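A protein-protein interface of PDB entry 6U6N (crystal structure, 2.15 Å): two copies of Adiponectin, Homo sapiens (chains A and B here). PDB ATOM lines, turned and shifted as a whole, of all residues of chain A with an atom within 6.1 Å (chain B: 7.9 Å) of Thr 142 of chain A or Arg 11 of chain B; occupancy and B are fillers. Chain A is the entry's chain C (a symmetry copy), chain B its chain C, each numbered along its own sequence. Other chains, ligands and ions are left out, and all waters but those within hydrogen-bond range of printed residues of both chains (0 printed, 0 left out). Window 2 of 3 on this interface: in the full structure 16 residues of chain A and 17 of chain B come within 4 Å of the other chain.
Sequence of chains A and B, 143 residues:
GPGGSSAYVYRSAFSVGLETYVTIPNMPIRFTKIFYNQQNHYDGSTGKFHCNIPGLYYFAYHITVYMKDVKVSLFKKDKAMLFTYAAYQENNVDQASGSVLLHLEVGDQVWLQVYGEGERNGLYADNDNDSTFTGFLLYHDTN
The guanidinium group (NH2) of Arg 11 of chain B sits at hydrogen-bond distance from the backbone carbonyl oxygen (O) of His 140 of chain A (2.5 Å).
NH2 of Arg 11 of chain B lies within hydrogen-bond range of OG1 of Thr 142 of chain A (3.3 Å).
The side-chain hydroxyl of Tyr 139 of chain A sits at hydrogen-bond distance from the backbone carbonyl oxygen of Ser 12 of chain B (3.4 Å).
The backbone carbonyl oxygen (O) of Leu 137 of chain B lies within hydrogen-bond range of the side-chain hydroxyl (OH) of Tyr 139 of chain A, 2.8 Å away.
OG of Ser 12 of chain B is in hydrogen-bond range of ND1 of His 41 of chain B (2.7 Å).
N of Leu 137 of chain B lies within hydrogen-bond range of O of Ser 12 of chain B (2.8 Å).
The backbone carbonyl oxygen (O) of Ala 13 of chain B sits close to the side-chain amide oxygen (OE1) of Gln 39 of chain B, at 3.3 Å.
OH of Tyr 36 of chain B lies within hydrogen-bond range of NE2 of Gln 38 of chain B (2.9 Å).
OH of Tyr 36 of chain B lies within hydrogen-bond range of NE2 of Gln 39 of chain B, at 3.0 Å.
N of Leu 56 of chain A lies within hydrogen-bond range of O of Tyr 139 of chain A (2.7 Å).
Among the printed residues, merely in contact across the chains: Leu 56 of chain A with Ala 13 of chain B (3.8 Å), Leu 56 of chain A with Tyr 36 of chain B (3.5 Å), Tyr 139 of chain A with Arg 11 of chain B (3.6 Å), Tyr 139 of chain A with Ala 13 of chain B (3.9 Å) and Asp 141 of chain A with Arg 11 of chain B (3.8 Å).
Printed residues of chain B within 4 Å of Tyr 139 of chain A: Arg 11 (3.6 Å), Ser 12 (3.4 Å), Ala 13 (3.9 Å) and Leu 137 (2.8 Å).
Of the printed residues of chain B, Asp 141 of chain A touches Arg 11.
Of chain B, only Arg 11 (3.3 Å) comes within 4 Å of Thr 142 of chain A.
Arg 11 of chain B touches just these residues of chain A: Tyr 139, His 140, Asp 141 and Thr 142.
Printed residues of chain A within 4 Å of Leu 137 of chain B: Tyr 139.
The nearest printed residue of chain B that does not touch Thr 142 of chain A is Gln 38 of chain B (8.1 Å).
The nearest residue of chain A that does not touch Arg 11 of chain B is Leu 56 of chain A (5.7 Å).
The nearest printed residue of chain A that does not touch Leu 137 of chain B is Leu 56 of chain A (8.0 Å).
Of the 7 printed residues of chain A, 5 touch a printed residue of chain B.
Printed residues of chain A that touch a printed residue of chain B: Leu 56, Tyr 139, His 140, Asp 141 and Thr 142.
Position printed for both chains: 140.
Of the 9 pairs that touch across the chains among the printed residues, none has its exchanged pair printed and touching as well.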
ATOM      1  N   GLY A  55      17.441  36.791  22.919  1.00  0.00           N
ATOM      2  CA  GLY A  55      16.984  35.600  23.599  1.00  0.00           C
ATOM      3  C   GLY A  55      15.916  35.928  24.624  1.00  0.00           C
ATOM      4  O   GLY A  55      15.385  37.037  24.669  1.00  0.00           O
ATOM      5  N   LEU A  56      15.615  34.923  25.443  1.00  0.00           N
ATOM      6  CA  LEU A  56      14.604  35.036  26.485  1.00  0.00           C
ATOM      7  C   LEU A  56      15.238  35.564  27.764  1.00  0.00           C
ATOM      8  O   LEU A  56      16.225  35.004  28.253  1.00  0.00           O
ATOM      9  CB  LEU A  56      13.947  33.679  26.743  1.00  0.00           C
ATOM     10  CG  LEU A  56      12.883  33.638  27.842  1.00  0.00           C
ATOM     11  CD1 LEU A  56      11.722  34.560  27.498  1.00  0.00           C
ATOM     12  CD2 LEU A  56      12.400  32.213  28.065  1.00  0.00           C
ATOM     13  N   TYR A 139      17.685  32.090  28.165  1.00  0.00           N
ATOM     14  CA  TYR A 139      17.937  31.293  26.969  1.00  0.00           C
ATOM     15  C   TYR A 139      18.356  32.228  25.846  1.00  0.00           C
ATOM     16  O   TYR A 139      17.627  33.169  25.519  1.00  0.00           O
ATOM     17  CB  TYR A 139      16.695  30.501  26.551  1.00  0.00           C
ATOM     18  CG  TYR A 139      16.145  29.550  27.592  1.00  0.00           C
ATOM     19  CD1 TYR A 139      16.984  28.895  28.484  1.00  0.00           C
ATOM     20  CD2 TYR A 139      14.781  29.300  27.672  1.00  0.00           C
ATOM     21  CE1 TYR A 139      16.474  28.020  29.432  1.00  0.00           C
ATOM     22  CE2 TYR A 139      14.264  28.431  28.613  1.00  0.00           C
ATOM     23  CZ  TYR A 139      15.114  27.793  29.490  1.00  0.00           C
ATOM     24  OH  TYR A 139      14.595  26.927  30.427  1.00  0.00           O
ATOM     25  N   HIS A 140      19.519  31.972  25.256  1.00  0.00           N
ATOM     26  CA  HIS A 140      19.954  32.731  24.096  1.00  0.00           C
ATOM     27  C   HIS A 140      19.475  32.047  22.821  1.00  0.00           C
ATOM     28  O   HIS A 140      19.386  30.819  22.747  1.00  0.00           O
ATOM     29  CB  HIS A 140      21.476  32.876  24.074  1.00  0.00           C
ATOM     30  CG  HIS A 140      22.197  31.632  23.667  1.00  0.00           C
ATOM     31  ND1 HIS A 140      22.525  31.356  22.356  1.00  0.00           N
ATOM     32  CD2 HIS A 140      22.652  30.585  24.396  1.00  0.00           C
ATOM     33  CE1 HIS A 140      23.151  30.195  22.295  1.00  0.00           C
ATOM     34  NE2 HIS A 140      23.241  29.706  23.519  1.00  0.00           N
ATOM     35  N   ASP A 141      19.155  32.860  21.817  1.00  0.00           N
ATOM     36  CA  ASP A 141      18.689  32.320  20.547  1.00  0.00           C
ATOM     37  C   ASP A 141      19.797  31.530  19.863  1.00  0.00           C
ATOM     38  O   ASP A 141      20.971  31.906  19.908  1.00  0.00           O
ATOM     39  CB  ASP A 141      18.207  33.448  19.633  1.00  0.00           C
ATOM     40  CG  ASP A 141      16.897  34.058  20.098  1.00  0.00           C
ATOM     41  OD1 ASP A 141      16.345  33.588  21.115  1.00  0.00           O
ATOM     42  OD2 ASP A 141      16.419  35.007  19.442  1.00  0.00           O
ATOM     43  N   THR A 142      19.417  30.424  19.227  1.00  0.00           N
ATOM     44  CA  THR A 142      20.350  29.560  18.509  1.00  0.00           C
ATOM     45  C   THR A 142      19.855  29.405  17.077  1.00  0.00           C
ATOM     46  O   THR A 142      18.889  28.675  16.825  1.00  0.00           O
ATOM     47  CB  THR A 142      20.484  28.199  19.193  1.00  0.00           C
ATOM     48  OG1 THR A 142      20.966  28.379  20.530  1.00  0.00           O
ATOM     49  CG2 THR A 142      21.456  27.314  18.425  1.00  0.00           C
ATOM     50  N   ASN A 143      20.514  30.088  16.147  1.00  0.00           N
ATOM     51  CA  ASN A 143      20.144  30.023  14.738  1.00  0.00           C
ATOM     52  C   ASN A 143      21.382  30.009  13.846  1.00  0.00           C
ATOM     53  O   ASN A 143      21.996  28.963  13.637  1.00  0.00           O
ATOM     54  CB  ASN A 143      19.240  31.200  14.366  1.00  0.00           C
ATOM     55  CG  ASN A 143      17.874  31.118  15.019  1.00  0.00           C
ATOM     56  OD1 ASN A 143      17.228  30.070  15.004  1.00  0.00           O
ATOM     57  ND2 ASN A 143      17.427  32.226  15.601  1.00  0.00           N
ATOM     58  N   TYR B  10      18.249  22.704  25.887  1.00  0.00           N
ATOM     59  CA  TYR B  10      17.044  22.308  26.604  1.00  0.00           C
ATOM     60  C   TYR B  10      16.295  23.547  27.081  1.00  0.00           C
ATOM     61  O   TYR B  10      16.762  24.259  27.974  1.00  0.00           O
ATOM     62  CB  TYR B  10      17.384  21.400  27.793  1.00  0.00           C
ATOM     63  CG  TYR B  10      18.317  20.248  27.477  1.00  0.00           C
ATOM     64  CD1 TYR B  10      19.700  20.427  27.474  1.00  0.00           C
ATOM     65  CD2 TYR B  10      17.822  18.975  27.201  1.00  0.00           C
ATOM     66  CE1 TYR B  10      20.564  19.376  27.192  1.00  0.00           C
ATOM     67  CE2 TYR B  10      18.681  17.912  26.920  1.00  0.00           C
ATOM     68  CZ  TYR B  10      20.052  18.120  26.918  1.00  0.00           C
ATOM     69  OH  TYR B  10      20.913  17.074  26.639  1.00  0.00           O
ATOM     70  N   ARG B  11      15.139  23.803  26.477  1.00  0.00           N
ATOM     71  CA  ARG B  11      14.319  24.963  26.789  1.00  0.00           C
ATOM     72  C   ARG B  11      12.935  24.518  27.227  1.00  0.00           C
ATOM     73  O   ARG B  11      12.340  23.623  26.620  1.00  0.00           O
ATOM     74  CB  ARG B  11      14.190  25.898  25.579  1.00  0.00           C
ATOM     75  CG  ARG B  11      15.481  26.565  25.123  1.00  0.00           C
ATOM     76  CD  ARG B  11      15.242  27.338  23.833  1.00  0.00           C
ATOM     77  NE  ARG B  11      16.463  27.534  23.054  1.00  0.00           N
ATOM     78  CZ  ARG B  11      16.938  28.722  22.692  1.00  0.00           C
ATOM     79  NH1 ARG B  11      16.290  29.826  23.030  1.00  0.00           N
ATOM     80  NH2 ARG B  11      18.055  28.808  21.980  1.00  0.00           N
ATOM     81  N   SER B  12      12.435  25.157  28.283  1.00  0.00           N
ATOM     82  CA  SER B  12      11.067  24.951  28.755  1.00  0.00           C
ATOM     83  C   SER B  12      10.767  26.076  29.732  1.00  0.00           C
ATOM     84  O   SER B  12      11.295  26.077  30.850  1.00  0.00           O
ATOM     85  CB  SER B  12      10.905  23.588  29.416  1.00  0.00           C
ATOM     86  OG  SER B  12       9.581  23.399  29.884  1.00  0.00           O
ATOM     87  N   ALA B  13       9.951  27.038  29.306  1.00  0.00           N
ATOM     88  CA  ALA B  13       9.651  28.205  30.117  1.00  0.00           C
ATOM     89  C   ALA B  13       8.263  28.708  29.757  1.00  0.00           C
ATOM     90  O   ALA B  13       7.689  28.328  28.734  1.00  0.00           O
ATOM     91  CB  ALA B  13      10.699  29.307  29.920  1.00  0.00           C
ATOM     92  N   TYR B  36       5.142  34.776  27.448  1.00  0.00           N
ATOM     93  CA  TYR B  36       6.039  33.864  26.757  1.00  0.00           C
ATOM     94  C   TYR B  36       5.489  32.448  26.855  1.00  0.00           C
ATOM     95  O   TYR B  36       5.046  32.018  27.923  1.00  0.00           O
ATOM     96  CB  TYR B  36       7.455  33.910  27.341  1.00  0.00           C
ATOM     97  CG  TYR B  36       8.414  32.948  26.675  1.00  0.00           C
ATOM     98  CD1 TYR B  36       8.644  31.685  27.204  1.00  0.00           C
ATOM     99  CD2 TYR B  36       9.083  33.304  25.511  1.00  0.00           C
ATOM    100  CE1 TYR B  36       9.516  30.804  26.594  1.00  0.00           C
ATOM    101  CE2 TYR B  36       9.957  32.432  24.898  1.00  0.00           C
ATOM    102  CZ  TYR B  36      10.171  31.183  25.443  1.00  0.00           C
ATOM    103  OH  TYR B  36      11.042  30.310  24.831  1.00  0.00           O
ATOM    104  N   GLN B  38       6.837  29.574  24.091  1.00  0.00           N
ATOM    105  CA  GLN B  38       7.329  29.089  22.807  1.00  0.00           C
ATOM    106  C   GLN B  38       7.370  27.570  22.729  1.00  0.00           C
ATOM    107  O   GLN B  38       7.176  27.007  21.645  1.00  0.00           O
ATOM    108  CB  GLN B  38       8.722  29.663  22.535  1.00  0.00           C
ATOM    109  CG  GLN B  38       9.305  29.300  21.178  1.00  0.00           C
ATOM    110  CD  GLN B  38      10.731  29.785  21.013  1.00  0.00           C
ATOM    111  OE1 GLN B  38      11.392  29.481  20.020  1.00  0.00           O
ATOM    112  NE2 GLN B  38      11.214  30.543  21.990  1.00  0.00           N
ATOM    113  N   GLN B  39       7.615  26.894  23.850  1.00  0.00           N
ATOM    114  CA  GLN B  39       7.598  25.438  23.894  1.00  0.00           C
ATOM    115  C   GLN B  39       6.192  24.874  24.036  1.00  0.00           C
ATOM    116  O   GLN B  39       6.019  23.656  23.928  1.00  0.00           O
ATOM    117  CB  GLN B  39       8.474  24.930  25.046  1.00  0.00           C
ATOM    118  CG  GLN B  39       9.933  25.368  24.979  1.00  0.00           C
ATOM    119  CD  GLN B  39      10.133  26.814  25.396  1.00  0.00           C
ATOM    120  OE1 GLN B  39       9.245  27.429  25.986  1.00  0.00           O
ATOM    121  NE2 GLN B  39      11.299  27.366  25.082  1.00  0.00           N
ATOM    122  N   ASN B  40       5.197  25.733  24.272  1.00  0.00           N
ATOM    123  CA  ASN B  40       3.799  25.325  24.421  1.00  0.00           C
ATOM    124  C   ASN B  40       3.637  24.292  25.536  1.00  0.00           C
ATOM    125  O   ASN B  40       2.959  23.275  25.380  1.00  0.00           O
ATOM    126  CB  ASN B  40       3.235  24.803  23.097  1.00  0.00           C
ATOM    127  CG  ASN B  40       3.274  25.847  21.998  1.00  0.00           C
ATOM    128  OD1 ASN B  40       3.923  25.658  20.969  1.00  0.00           O
ATOM    129  ND2 ASN B  40       2.587  26.963  22.216  1.00  0.00           N
ATOM    130  N   HIS B  41       4.274  24.565  26.675  1.00  0.00           N
ATOM    131  CA  HIS B  41       4.167  23.709  27.848  1.00  0.00           C
ATOM    132  C   HIS B  41       3.181  24.236  28.883  1.00  0.00           C
ATOM    133  O   HIS B  41       2.894  23.530  29.855  1.00  0.00           O
ATOM    134  CB  HIS B  41       5.544  23.524  28.496  1.00  0.00           C
ATOM    135  CG  HIS B  41       6.505  22.746  27.653  1.00  0.00           C
ATOM    136  ND1 HIS B  41       7.862  22.734  27.888  1.00  0.00           N
ATOM    137  CD2 HIS B  41       6.303  21.951  26.576  1.00  0.00           C
ATOM    138  CE1 HIS B  41       8.456  21.966  26.991  1.00  0.00           C
ATOM    139  NE2 HIS B  41       7.531  21.480  26.182  1.00  0.00           N
ATOM    140  N   ASN B  52       7.732  18.545  30.369  1.00  0.00           N
ATOM    141  CA  ASN B  52       8.189  17.595  29.367  1.00  0.00           C
ATOM    142  C   ASN B  52       9.689  17.348  29.408  1.00  0.00           C
ATOM    143  O   ASN B  52      10.161  16.417  28.745  1.00  0.00           O
ATOM    144  CB  ASN B  52       7.798  18.062  27.955  1.00  0.00           C
ATOM    145  CG  ASN B  52       6.418  17.583  27.546  1.00  0.00           C
ATOM    146  OD1 ASN B  52       5.411  18.233  27.828  1.00  0.00           O
ATOM    147  ND2 ASN B  52       6.365  16.438  26.874  1.00  0.00           N
ATOM    148  N   ILE B  53      10.446  18.143  30.156  1.00  0.00           N
ATOM    149  CA  ILE B  53      11.876  17.945  30.344  1.00  0.00           C
ATOM    150  C   ILE B  53      12.124  17.805  31.841  1.00  0.00           C
ATOM    151  O   ILE B  53      11.864  18.744  32.599  1.00  0.00           O
ATOM    152  CB  ILE B  53      12.708  19.101  29.763  1.00  0.00           C
ATOM    153  CG1 ILE B  53      12.319  19.362  28.305  1.00  0.00           C
ATOM    154  CG2 ILE B  53      14.193  18.791  29.872  1.00  0.00           C
ATOM    155  CD1 ILE B  53      13.084  20.503  27.666  1.00  0.00           C
ATOM    156  N   TYR B  57      13.143  23.230  38.294  1.00  0.00           N
ATOM    157  CA  TYR B  57      12.394  24.343  37.729  1.00  0.00           C
ATOM    158  C   TYR B  57      12.213  25.436  38.772  1.00  0.00           C
ATOM    159  O   TYR B  57      12.019  25.151  39.957  1.00  0.00           O
ATOM    160  CB  TYR B  57      11.025  23.881  37.218  1.00  0.00           C
ATOM    161  CG  TYR B  57      11.094  23.087  35.935  1.00  0.00           C
ATOM    162  CD1 TYR B  57      11.506  21.761  35.938  1.00  0.00           C
ATOM    163  CD2 TYR B  57      10.747  23.664  34.722  1.00  0.00           C
ATOM    164  CE1 TYR B  57      11.573  21.033  34.767  1.00  0.00           C
ATOM    165  CE2 TYR B  57      10.809  22.945  33.547  1.00  0.00           C
ATOM    166  CZ  TYR B  57      11.224  21.632  33.573  1.00  0.00           C
ATOM    167  OH  TYR B  57      11.284  20.916  32.399  1.00  0.00           O
ATOM    168  N   PHE B 136      10.432  28.299  34.653  1.00  0.00           N
ATOM    169  CA  PHE B 136      11.392  27.946  33.618  1.00  0.00           C
ATOM    170  C   PHE B 136      12.326  26.857  34.124  1.00  0.00           C
ATOM    171  O   PHE B 136      12.558  26.725  35.329  1.00  0.00           O
ATOM    172  CB  PHE B 136      12.194  29.166  33.145  1.00  0.00           C
ATOM    173  CG  PHE B 136      12.931  29.891  34.242  1.00  0.00           C
ATOM    174  CD1 PHE B 136      14.210  29.507  34.611  1.00  0.00           C
ATOM    175  CD2 PHE B 136      12.356  30.979  34.880  1.00  0.00           C
ATOM    176  CE1 PHE B 136      14.892  30.179  35.608  1.00  0.00           C
ATOM    177  CE2 PHE B 136      13.034  31.657  35.877  1.00  0.00           C
ATOM    178  CZ  PHE B 136      14.304  31.255  36.242  1.00  0.00           C
ATOM    179  N   LEU B 137      12.860  26.088  33.177  1.00  0.00           N
ATOM    180  CA  LEU B 137      13.799  25.016  33.480  1.00  0.00           C
ATOM    181  C   LEU B 137      15.170  25.608  33.783  1.00  0.00           C
ATOM    182  O   LEU B 137      15.793  26.224  32.913  1.00  0.00           O
ATOM    183  CB  LEU B 137      13.885  24.040  32.309  1.00  0.00           C
ATOM    184  CG  LEU B 137      15.000  22.993  32.370  1.00  0.00           C
ATOM    185  CD1 LEU B 137      14.826  22.086  33.578  1.00  0.00           C
ATOM    186  CD2 LEU B 137      15.040  22.180  31.087  1.00  0.00           C
ATOM    187  N   HIS B 140      18.541  20.861  33.838  1.00  0.00           N
ATOM    188  CA  HIS B 140      17.960  19.637  33.311  1.00  0.00           C
ATOM    189  C   HIS B 140      18.736  18.432  33.827  1.00  0.00           C
ATOM    190  O   HIS B 140      19.952  18.492  34.028  1.00  0.00           O
ATOM    191  CB  HIS B 140      17.957  19.645  31.782  1.00  0.00           C
ATOM    192  CG  HIS B 140      19.301  19.399  31.173  1.00  0.00           C
ATOM    193  ND1 HIS B 140      19.750  18.137  30.847  1.00  0.00           N
ATOM    194  CD2 HIS B 140      20.296  20.252  30.832  1.00  0.00           C
ATOM    195  CE1 HIS B 140      20.963  18.223  30.332  1.00  0.00           C
ATOM    196  NE2 HIS B 140      21.318  19.496  30.311  1.00  0.00           N
